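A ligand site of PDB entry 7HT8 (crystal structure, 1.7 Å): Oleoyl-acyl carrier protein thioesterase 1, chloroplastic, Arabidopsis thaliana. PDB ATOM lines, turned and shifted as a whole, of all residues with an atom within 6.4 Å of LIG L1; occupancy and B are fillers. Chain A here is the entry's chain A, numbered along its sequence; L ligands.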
ATOM      1  N   GLY A  41      -8.779  18.733  -5.479  1.00  0.00           N
ATOM      2  CA  GLY A  41      -8.655  17.284  -5.585  1.00  0.00           C
ATOM      3  C   GLY A  41      -9.475  16.733  -6.754  1.00  0.00           C
ATOM      4  O   GLY A  41      -9.008  15.874  -7.494  1.00  0.00           O
ATOM      5  N   HIS A  44      -7.854  17.742 -10.066  1.00  0.00           N
ATOM      6  CA  HIS A  44      -6.710  16.862 -10.295  1.00  0.00           C
ATOM      7  C   HIS A  44      -7.164  15.518 -10.929  1.00  0.00           C
ATOM      8  O   HIS A  44      -6.613  15.114 -11.938  1.00  0.00           O
ATOM      9  CB  HIS A  44      -5.931  16.562  -8.977  1.00  0.00           C
ATOM     10  CG  HIS A  44      -4.737  15.665  -9.137  1.00  0.00           C
ATOM     11  ND1 HIS A  44      -4.206  14.970  -8.063  1.00  0.00           N
ATOM     12  CD2 HIS A  44      -4.017  15.365 -10.251  1.00  0.00           C
ATOM     13  CE1 HIS A  44      -3.189  14.291  -8.555  1.00  0.00           C
ATOM     14  NE2 HIS A  44      -3.045  14.487  -9.863  1.00  0.00           N
ATOM     15  N   ALA A  45      -8.174  14.862 -10.358  1.00  0.00           N
ATOM     16  CA  ALA A  45      -8.699  13.582 -10.877  1.00  0.00           C
ATOM     17  C   ALA A  45      -9.213  13.720 -12.313  1.00  0.00           C
ATOM     18  O   ALA A  45      -8.896  12.890 -13.179  1.00  0.00           O
ATOM     19  CB  ALA A  45      -9.786  13.057  -9.946  1.00  0.00           C
ATOM     20  N   GLN A  46      -9.931  14.807 -12.609  1.00  0.00           N
ATOM     21  CA  GLN A  46     -10.466  15.043 -13.953  1.00  0.00           C
ATOM     22  C   GLN A  46      -9.369  15.281 -14.981  1.00  0.00           C
ATOM     23  O   GLN A  46      -9.465  14.797 -16.119  1.00  0.00           O
ATOM     24  CB  GLN A  46     -11.440  16.230 -13.959  1.00  0.00           C
ATOM     25  CG  GLN A  46     -12.747  15.980 -13.227  1.00  0.00           C
ATOM     26  CD  GLN A  46     -13.631  17.209 -13.154  1.00  0.00           C
ATOM     27  OE1 GLN A  46     -13.552  18.018 -12.221  1.00  0.00           O
ATOM     28  NE2 GLN A  46     -14.535  17.365 -14.119  1.00  0.00           N
ATOM     29  N   VAL A  48      -6.354  14.084 -15.075  1.00  0.00           N
ATOM     30  CA  VAL A  48      -5.597  12.884 -15.409  1.00  0.00           C
ATOM     31  C   VAL A  48      -6.499  11.758 -15.959  1.00  0.00           C
ATOM     32  O   VAL A  48      -6.091  10.599 -15.961  1.00  0.00           O
ATOM     33  CB  VAL A  48      -4.692  12.397 -14.272  1.00  0.00           C
ATOM     34  CG1 VAL A  48      -3.715  13.494 -13.847  1.00  0.00           C
ATOM     35  CG2 VAL A  48      -5.510  11.923 -13.077  1.00  0.00           C
ATOM     36  N   PHE A  50      -9.911  10.826 -15.099  1.00  0.00           N
ATOM     37  CA  PHE A  50     -11.040  10.196 -14.400  1.00  0.00           C
ATOM     38  C   PHE A  50     -12.388  10.806 -14.832  1.00  0.00           C
ATOM     39  O   PHE A  50     -12.467  11.979 -15.174  1.00  0.00           O
ATOM     40  CB  PHE A  50     -10.853  10.164 -12.862  1.00  0.00           C
ATOM     41  CG  PHE A  50      -9.698   9.263 -12.471  1.00  0.00           C
ATOM     42  CD1 PHE A  50      -8.408   9.753 -12.406  1.00  0.00           C
ATOM     43  CD2 PHE A  50      -9.892   7.900 -12.295  1.00  0.00           C
ATOM     44  CE1 PHE A  50      -7.349   8.908 -12.096  1.00  0.00           C
ATOM     45  CE2 PHE A  50      -8.827   7.076 -11.991  1.00  0.00           C
ATOM     46  CZ  PHE A  50      -7.566   7.581 -11.894  1.00  0.00           C
ATOM     47  N   ALA A  56     -13.210   9.399  -8.377  1.00  0.00           N
ATOM     48  CA  ALA A  56     -11.911   9.122  -8.984  1.00  0.00           C
ATOM     49  C   ALA A  56     -11.617   7.618  -9.026  1.00  0.00           C
ATOM     50  O   ALA A  56     -10.581   7.145  -8.562  1.00  0.00           O
ATOM     51  CB  ALA A  56     -10.817   9.865  -8.238  1.00  0.00           C
ATOM     52  N   TRP A  68     -13.521   5.119  -3.201  1.00  0.00           N
ATOM     53  CA  TRP A  68     -12.543   5.622  -2.252  1.00  0.00           C
ATOM     54  C   TRP A  68     -13.294   6.315  -1.142  1.00  0.00           C
ATOM     55  O   TRP A  68     -14.216   7.075  -1.428  1.00  0.00           O
ATOM     56  CB  TRP A  68     -11.650   6.691  -2.927  1.00  0.00           C
ATOM     57  CG  TRP A  68     -10.647   6.101  -3.858  1.00  0.00           C
ATOM     58  CD1 TRP A  68     -10.640   6.155  -5.223  1.00  0.00           C
ATOM     59  CD2 TRP A  68      -9.511   5.319  -3.488  1.00  0.00           C
ATOM     60  NE1 TRP A  68      -9.558   5.485  -5.726  1.00  0.00           N
ATOM     61  CE2 TRP A  68      -8.849   4.952  -4.679  1.00  0.00           C
ATOM     62  CE3 TRP A  68      -8.972   4.917  -2.261  1.00  0.00           C
ATOM     63  CZ2 TRP A  68      -7.709   4.150  -4.677  1.00  0.00           C
ATOM     64  CZ3 TRP A  68      -7.853   4.119  -2.265  1.00  0.00           C
ATOM     65  CH2 TRP A  68      -7.225   3.754  -3.463  1.00  0.00           C
ATOM     66  N   TRP A  92      -1.386  16.234  -4.591  1.00  0.00           N
ATOM     67  CA  TRP A  92      -0.830  15.043  -5.205  1.00  0.00           C
ATOM     68  C   TRP A  92      -1.281  13.848  -4.387  1.00  0.00           C
ATOM     69  O   TRP A  92      -1.671  13.983  -3.215  1.00  0.00           O
ATOM     70  CB  TRP A  92       0.719  15.145  -5.304  1.00  0.00           C
ATOM     71  CG  TRP A  92       1.411  15.132  -3.957  1.00  0.00           C
ATOM     72  CD1 TRP A  92       1.857  14.042  -3.277  1.00  0.00           C
ATOM     73  CD2 TRP A  92       1.782  16.278  -3.180  1.00  0.00           C
ATOM     74  NE1 TRP A  92       2.421  14.430  -2.087  1.00  0.00           N
ATOM     75  CE2 TRP A  92       2.396  15.806  -2.001  1.00  0.00           C
ATOM     76  CE3 TRP A  92       1.600  17.671  -3.337  1.00  0.00           C
ATOM     77  CZ2 TRP A  92       2.911  16.663  -1.026  1.00  0.00           C
ATOM     78  CZ3 TRP A  92       2.087  18.512  -2.362  1.00  0.00           C
ATOM     79  CH2 TRP A  92       2.695  18.015  -1.208  1.00  0.00           C
ATOM     80  N   CYS A  93      -1.221  12.667  -4.989  1.00  0.00           N
ATOM     81  CA  CYS A  93      -1.568  11.433  -4.287  1.00  0.00           C
ATOM     82  C   CYS A  93      -0.355  10.523  -4.159  1.00  0.00           C
ATOM     83  O   CYS A  93       0.564  10.600  -4.980  1.00  0.00           O
ATOM     84  CB  CYS A  93      -2.701  10.715  -4.995  1.00  0.00           C
ATOM     85  SG  CYS A  93      -4.268  11.586  -4.915  1.00  0.00           S
ATOM     86  N   GLN A  94      -0.373   9.620  -3.175  1.00  0.00           N
ATOM     87  CA  GLN A  94       0.691   8.626  -3.041  1.00  0.00           C
ATOM     88  C   GLN A  94       0.141   7.339  -2.513  1.00  0.00           C
ATOM     89  O   GLN A  94      -0.681   7.351  -1.605  1.00  0.00           O
ATOM     90  CB  GLN A  94       1.824   9.110  -2.139  1.00  0.00           C
ATOM     91  CG  GLN A  94       2.908   9.878  -2.860  1.00  0.00           C
ATOM     92  CD  GLN A  94       4.251   9.546  -2.271  1.00  0.00           C
ATOM     93  OE1 GLN A  94       4.542   9.820  -1.090  1.00  0.00           O
ATOM     94  NE2 GLN A  94       5.113   8.950  -3.079  1.00  0.00           N
ATOM     95  N   THR A 101      -4.412   4.881   0.202  1.00  0.00           N
ATOM     96  CA  THR A 101      -3.710   5.984  -0.438  1.00  0.00           C
ATOM     97  C   THR A 101      -3.847   7.283   0.356  1.00  0.00           C
ATOM     98  O   THR A 101      -4.755   7.459   1.171  1.00  0.00           O
ATOM     99  CB  THR A 101      -4.219   6.157  -1.885  1.00  0.00           C
ATOM    100  OG1 THR A 101      -5.590   6.503  -1.830  1.00  0.00           O
ATOM    101  CG2 THR A 101      -4.051   4.902  -2.730  1.00  0.00           C
ATOM    102  N   ARG A 102      -2.951   8.200   0.094  1.00  0.00           N
ATOM    103  CA  ARG A 102      -2.904   9.472   0.763  1.00  0.00           C
ATOM    104  C   ARG A 102      -2.999  10.592  -0.283  1.00  0.00           C
ATOM    105  O   ARG A 102      -2.392  10.488  -1.345  1.00  0.00           O
ATOM    106  CB  ARG A 102      -1.558   9.539   1.491  1.00  0.00           C
ATOM    107  CG  ARG A 102      -1.461  10.521   2.618  1.00  0.00           C
ATOM    108  CD  ARG A 102      -0.074  10.548   3.217  1.00  0.00           C
ATOM    109  NE  ARG A 102       0.834  11.347   2.406  1.00  0.00           N
ATOM    110  CZ  ARG A 102       1.833  10.870   1.675  1.00  0.00           C
ATOM    111  NH1 ARG A 102       2.587  11.681   0.957  1.00  0.00           N
ATOM    112  NH2 ARG A 102       2.102   9.564   1.671  1.00  0.00           N
ATOM    113  N   ARG A 103      -3.763  11.657  -0.014  1.00  0.00           N
ATOM    114  CA  ARG A 103      -3.758  12.846  -0.836  1.00  0.00           C
ATOM    115  C   ARG A 103      -3.267  13.926   0.094  1.00  0.00           C
ATOM    116  O   ARG A 103      -3.822  14.097   1.188  1.00  0.00           O
ATOM    117  CB  ARG A 103      -5.141  13.223  -1.436  1.00  0.00           C
ATOM    118  CG  ARG A 103      -5.127  14.597  -2.113  1.00  0.00           C
ATOM    119  CD  ARG A 103      -6.430  14.878  -2.816  1.00  0.00           C
ATOM    120  NE  ARG A 103      -6.653  14.011  -3.974  1.00  0.00           N
ATOM    121  CZ  ARG A 103      -6.103  14.224  -5.172  1.00  0.00           C
ATOM    122  NH1 ARG A 103      -6.348  13.385  -6.172  1.00  0.00           N
ATOM    123  NH2 ARG A 103      -5.312  15.264  -5.377  1.00  0.00           N
ATOM    124  N   TRP A 105      -1.814  18.180   0.379  1.00  0.00           N
ATOM    125  CA  TRP A 105      -1.999  19.502  -0.184  1.00  0.00           C
ATOM    126  C   TRP A 105      -1.037  20.463   0.486  1.00  0.00           C
ATOM    127  O   TRP A 105      -0.684  20.288   1.654  1.00  0.00           O
ATOM    128  CB  TRP A 105      -3.430  20.036   0.087  1.00  0.00           C
ATOM    129  CG  TRP A 105      -4.599  19.299  -0.515  1.00  0.00           C
ATOM    130  CD1 TRP A 105      -5.331  19.714  -1.594  1.00  0.00           C
ATOM    131  CD2 TRP A 105      -5.353  18.236   0.101  1.00  0.00           C
ATOM    132  NE1 TRP A 105      -6.463  18.937  -1.726  1.00  0.00           N
ATOM    133  CE2 TRP A 105      -6.481  17.997  -0.719  1.00  0.00           C
ATOM    134  CE3 TRP A 105      -5.166  17.447   1.241  1.00  0.00           C
ATOM    135  CZ2 TRP A 105      -7.440  17.038  -0.392  1.00  0.00           C
ATOM    136  CZ3 TRP A 105      -6.124  16.514   1.581  1.00  0.00           C
ATOM    137  CH2 TRP A 105      -7.216  16.267   0.728  1.00  0.00           C
ATOM    138  N   SER A 121      -4.668  13.555   3.888  1.00  0.00           N
ATOM    139  CA  SER A 121      -5.852  12.714   4.087  1.00  0.00           C
ATOM    140  C   SER A 121      -5.490  11.262   3.806  1.00  0.00           C
ATOM    141  O   SER A 121      -4.692  10.994   2.901  1.00  0.00           O
ATOM    142  CB  SER A 121      -6.963  13.151   3.138  1.00  0.00           C
ATOM    143  OG  SER A 121      -6.486  13.167   1.796  1.00  0.00           O
ATOM    144  N   TRP A 123      -7.073   7.570   2.756  1.00  0.00           N
ATOM    145  CA  TRP A 123      -8.169   6.998   2.008  1.00  0.00           C
ATOM    146  C   TRP A 123      -8.049   5.468   1.950  1.00  0.00           C
ATOM    147  O   TRP A 123      -6.942   4.918   1.863  1.00  0.00           O
ATOM    148  CB  TRP A 123      -8.140   7.533   0.556  1.00  0.00           C
ATOM    149  CG  TRP A 123      -8.348   9.013   0.398  1.00  0.00           C
ATOM    150  CD1 TRP A 123      -7.433  10.006   0.577  1.00  0.00           C
ATOM    151  CD2 TRP A 123      -9.563   9.650   0.017  1.00  0.00           C
ATOM    152  NE1 TRP A 123      -8.005  11.240   0.328  1.00  0.00           N
ATOM    153  CE2 TRP A 123      -9.329  11.044   0.010  1.00  0.00           C
ATOM    154  CE3 TRP A 123     -10.844   9.181  -0.299  1.00  0.00           C
ATOM    155  CZ2 TRP A 123     -10.324  11.965  -0.311  1.00  0.00           C
ATOM    156  CZ3 TRP A 123     -11.828  10.097  -0.595  1.00  0.00           C
ATOM    157  CH2 TRP A 123     -11.555  11.466  -0.639  1.00  0.00           C
ATOM    158  N   TYR A 144      -3.230   3.066 -10.642  1.00  0.00           N
ATOM    159  CA  TYR A 144      -3.110   4.398 -10.031  1.00  0.00           C
ATOM    160  C   TYR A 144      -1.700   4.911  -9.927  1.00  0.00           C
ATOM    161  O   TYR A 144      -1.507   6.117  -9.924  1.00  0.00           O
ATOM    162  CB  TYR A 144      -3.716   4.408  -8.627  1.00  0.00           C
ATOM    163  CG  TYR A 144      -5.211   4.520  -8.640  1.00  0.00           C
ATOM    164  CD1 TYR A 144      -5.827   5.753  -8.791  1.00  0.00           C
ATOM    165  CD2 TYR A 144      -6.021   3.404  -8.521  1.00  0.00           C
ATOM    166  CE1 TYR A 144      -7.207   5.873  -8.804  1.00  0.00           C
ATOM    167  CE2 TYR A 144      -7.406   3.503  -8.528  1.00  0.00           C
ATOM    168  CZ  TYR A 144      -8.000   4.743  -8.688  1.00  0.00           C
ATOM    169  OH  TYR A 144      -9.359   4.866  -8.741  1.00  0.00           O
ATOM    170  N   PHE A 147      -0.072   7.886 -11.924  1.00  0.00           N
ATOM    171  CA  PHE A 147      -0.458   9.258 -11.612  1.00  0.00           C
ATOM    172  C   PHE A 147       0.182   9.820 -10.323  1.00  0.00           C
ATOM    173  O   PHE A 147      -0.102  10.956  -9.956  1.00  0.00           O
ATOM    174  CB  PHE A 147      -2.001   9.351 -11.489  1.00  0.00           C
ATOM    175  CG  PHE A 147      -2.704   8.789 -12.695  1.00  0.00           C
ATOM    176  CD1 PHE A 147      -2.526   9.360 -13.946  1.00  0.00           C
ATOM    177  CD2 PHE A 147      -3.461   7.637 -12.607  1.00  0.00           C
ATOM    178  CE1 PHE A 147      -3.122   8.812 -15.070  1.00  0.00           C
ATOM    179  CE2 PHE A 147      -4.088   7.102 -13.731  1.00  0.00           C
ATOM    180  CZ  PHE A 147      -3.918   7.698 -14.949  1.00  0.00           C
ATOM    181  N   CYS A 148       1.059   9.048  -9.667  1.00  0.00           N
ATOM    182  CA  CYS A 148       1.629   9.443  -8.392  1.00  0.00           C
ATOM    183  C   CYS A 148       3.163   9.539  -8.438  1.00  0.00           C
ATOM    184  O   CYS A 148       3.793   8.678  -9.069  1.00  0.00           O
ATOM    185  CB  CYS A 148       1.206   8.434  -7.318  1.00  0.00           C
ATOM    186  SG  CYS A 148      -0.583   8.232  -7.129  1.00  0.00           S
HETATM  187  N1  LIG L   1      -5.921   9.127  -7.610  1.00  0.00           N
HETATM  188  C1  LIG L   1      -4.039  10.432  -8.521  1.00  0.00           C
HETATM  189  C2  LIG L   1      -5.094  11.477  -8.884  1.00  0.00           C
HETATM  190  C3  LIG L   1      -6.381  10.830  -9.369  1.00  0.00           C
HETATM  191  C4  LIG L   1      -6.958   9.878  -8.334  1.00  0.00           C
HETATM  192  C5  LIG L   1      -8.128  11.659  -3.197  1.00  0.00           C
HETATM  193  O1  LIG L   1      -8.417  11.256  -5.750  1.00  0.00           O
HETATM  194  S1  LIG L   1      -8.550  10.568  -4.505  1.00  0.00           S
HETATM  195  O2  LIG L   1      -9.819   9.970  -4.210  1.00  0.00           O
HETATM  196  N2  LIG L   1      -7.465   9.365  -4.503  1.00  0.00           N
HETATM  197  C6  LIG L   1      -7.545   8.459  -3.359  1.00  0.00           C
HETATM  198  C7  LIG L   1      -7.440   8.593  -5.747  1.00  0.00           C
HETATM  199  C8  LIG L   1      -6.055   8.580  -6.389  1.00  0.00           C
HETATM  200  O3  LIG L   1      -5.086   8.147  -5.771  1.00  0.00           O
HETATM  201  C9  LIG L   1      -4.643   9.047  -8.337  1.00  0.00           C
HETATM  202  N1  LG2 L   2     -11.990  15.041  -2.228  1.00  0.00           N
HETATM  203  C1  LG2 L   2     -10.857  14.190  -4.268  1.00  0.00           C
HETATM  204  C2  LG2 L   2     -12.054  13.256  -4.406  1.00  0.00           C
HETATM  205  C3  LG2 L   2     -13.353  13.948  -4.009  1.00  0.00           C
HETATM  206  C4  LG2 L   2     -13.292  14.441  -2.570  1.00  0.00           C
HETATM  207  C5  LG2 L   2     -11.432  18.162   2.073  1.00  0.00           C
HETATM  208  O1  LG2 L   2     -13.684  17.186   1.259  1.00  0.00           O
HETATM  209  S1  LG2 L   2     -12.576  16.840   2.103  1.00  0.00           S
HETATM  210  O2  LG2 L   2     -12.818  16.499   3.470  1.00  0.00           O
HETATM  211  N2  LG2 L   2     -11.820  15.559   1.399  1.00  0.00           N
HETATM  212  C6  LG2 L   2     -11.453  14.464   2.301  1.00  0.00           C
HETATM  213  C7  LG2 L   2     -12.482  15.067   0.190  1.00  0.00           C
HETATM  214  C8  LG2 L   2     -11.547  15.288  -0.984  1.00  0.00           C
HETATM  215  O3  LG2 L   2     -10.415  15.732  -0.798  1.00  0.00           O
HETATM  216  C9  LG2 L   2     -11.180  15.393  -3.406  1.00  0.00           C
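The guanidinium group of Arg 103 sits at hydrogen-bond distance from an oxygen (O1) of LIG L1 (3.0 Å).
SG of Cys 93 sits close to O3 of LIG L1 (3.6 Å).
The guanidinium group (NH2) of Arg 103 sits at hydrogen-bond distance from a ring nitrogen (ND1) of His 44, at 2.9 Å.
The side-chain sulfur (SG) of Cys 93 is in hydrogen-bond range of the guanidinium group (NH1) of Arg 103 (3.0 Å).
The backbone NH (N) of Trp 123 lies within hydrogen-bond range of the backbone carbonyl oxygen (O) of Thr 101 (2.8 Å).
The backbone NH of Phe 50 lies within hydrogen-bond range of the backbone carbonyl oxygen of Ala 45 (3.0 Å).
NE1 of Trp 68 lies within hydrogen-bond range of OH of Tyr 144 (3.1 Å).
OH of Tyr 144 is in hydrogen-bond range of O of Ala 56 (2.6 Å).
O of Cys 93 lies close to SG of Cys 148, at 3.4 Å.
The indole nitrogen (NE1) of Trp 68 is in hydrogen-bond range of the backbone carbonyl oxygen (O) of Ala 56 (3.4 Å).
His 44 touches LIG L1 (CE1 to C2, 3.4 Å).
Ala 45 touches LIG L1.
Val 48 touches LIG L1 (CG2 to C3, 3.96 Å).
Phe 50 touches LIG L1 (CE1 to C3, 3.5 Å).
CB of Ala 56 touches O1 of LIG L1 (3.7 Å).
CD2 of Trp 68 touches C6 of LIG L1, 3.7 Å away.
Thr 101 touches LIG L1 (OG1 to C6, 3.2 Å).
Trp 123 touches LIG L1.
CD1 of Tyr 144 touches C9 of LIG L1 (3.5 Å).
CB of Phe 147 touches C1 of LIG L1, 3.8 Å away.
Hydrophobic or aromatic side chains that line LIG L1: His 44, Val 48, Phe 50, Ala 56, Trp 68, Trp 123, Tyr 144 and Phe 147.
Of the 20 residues printed, 12 come within 4 Å of LIG L1.
The nearest printed residue that does not touch LIG L1 is Cys 148 (4.3 Å).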
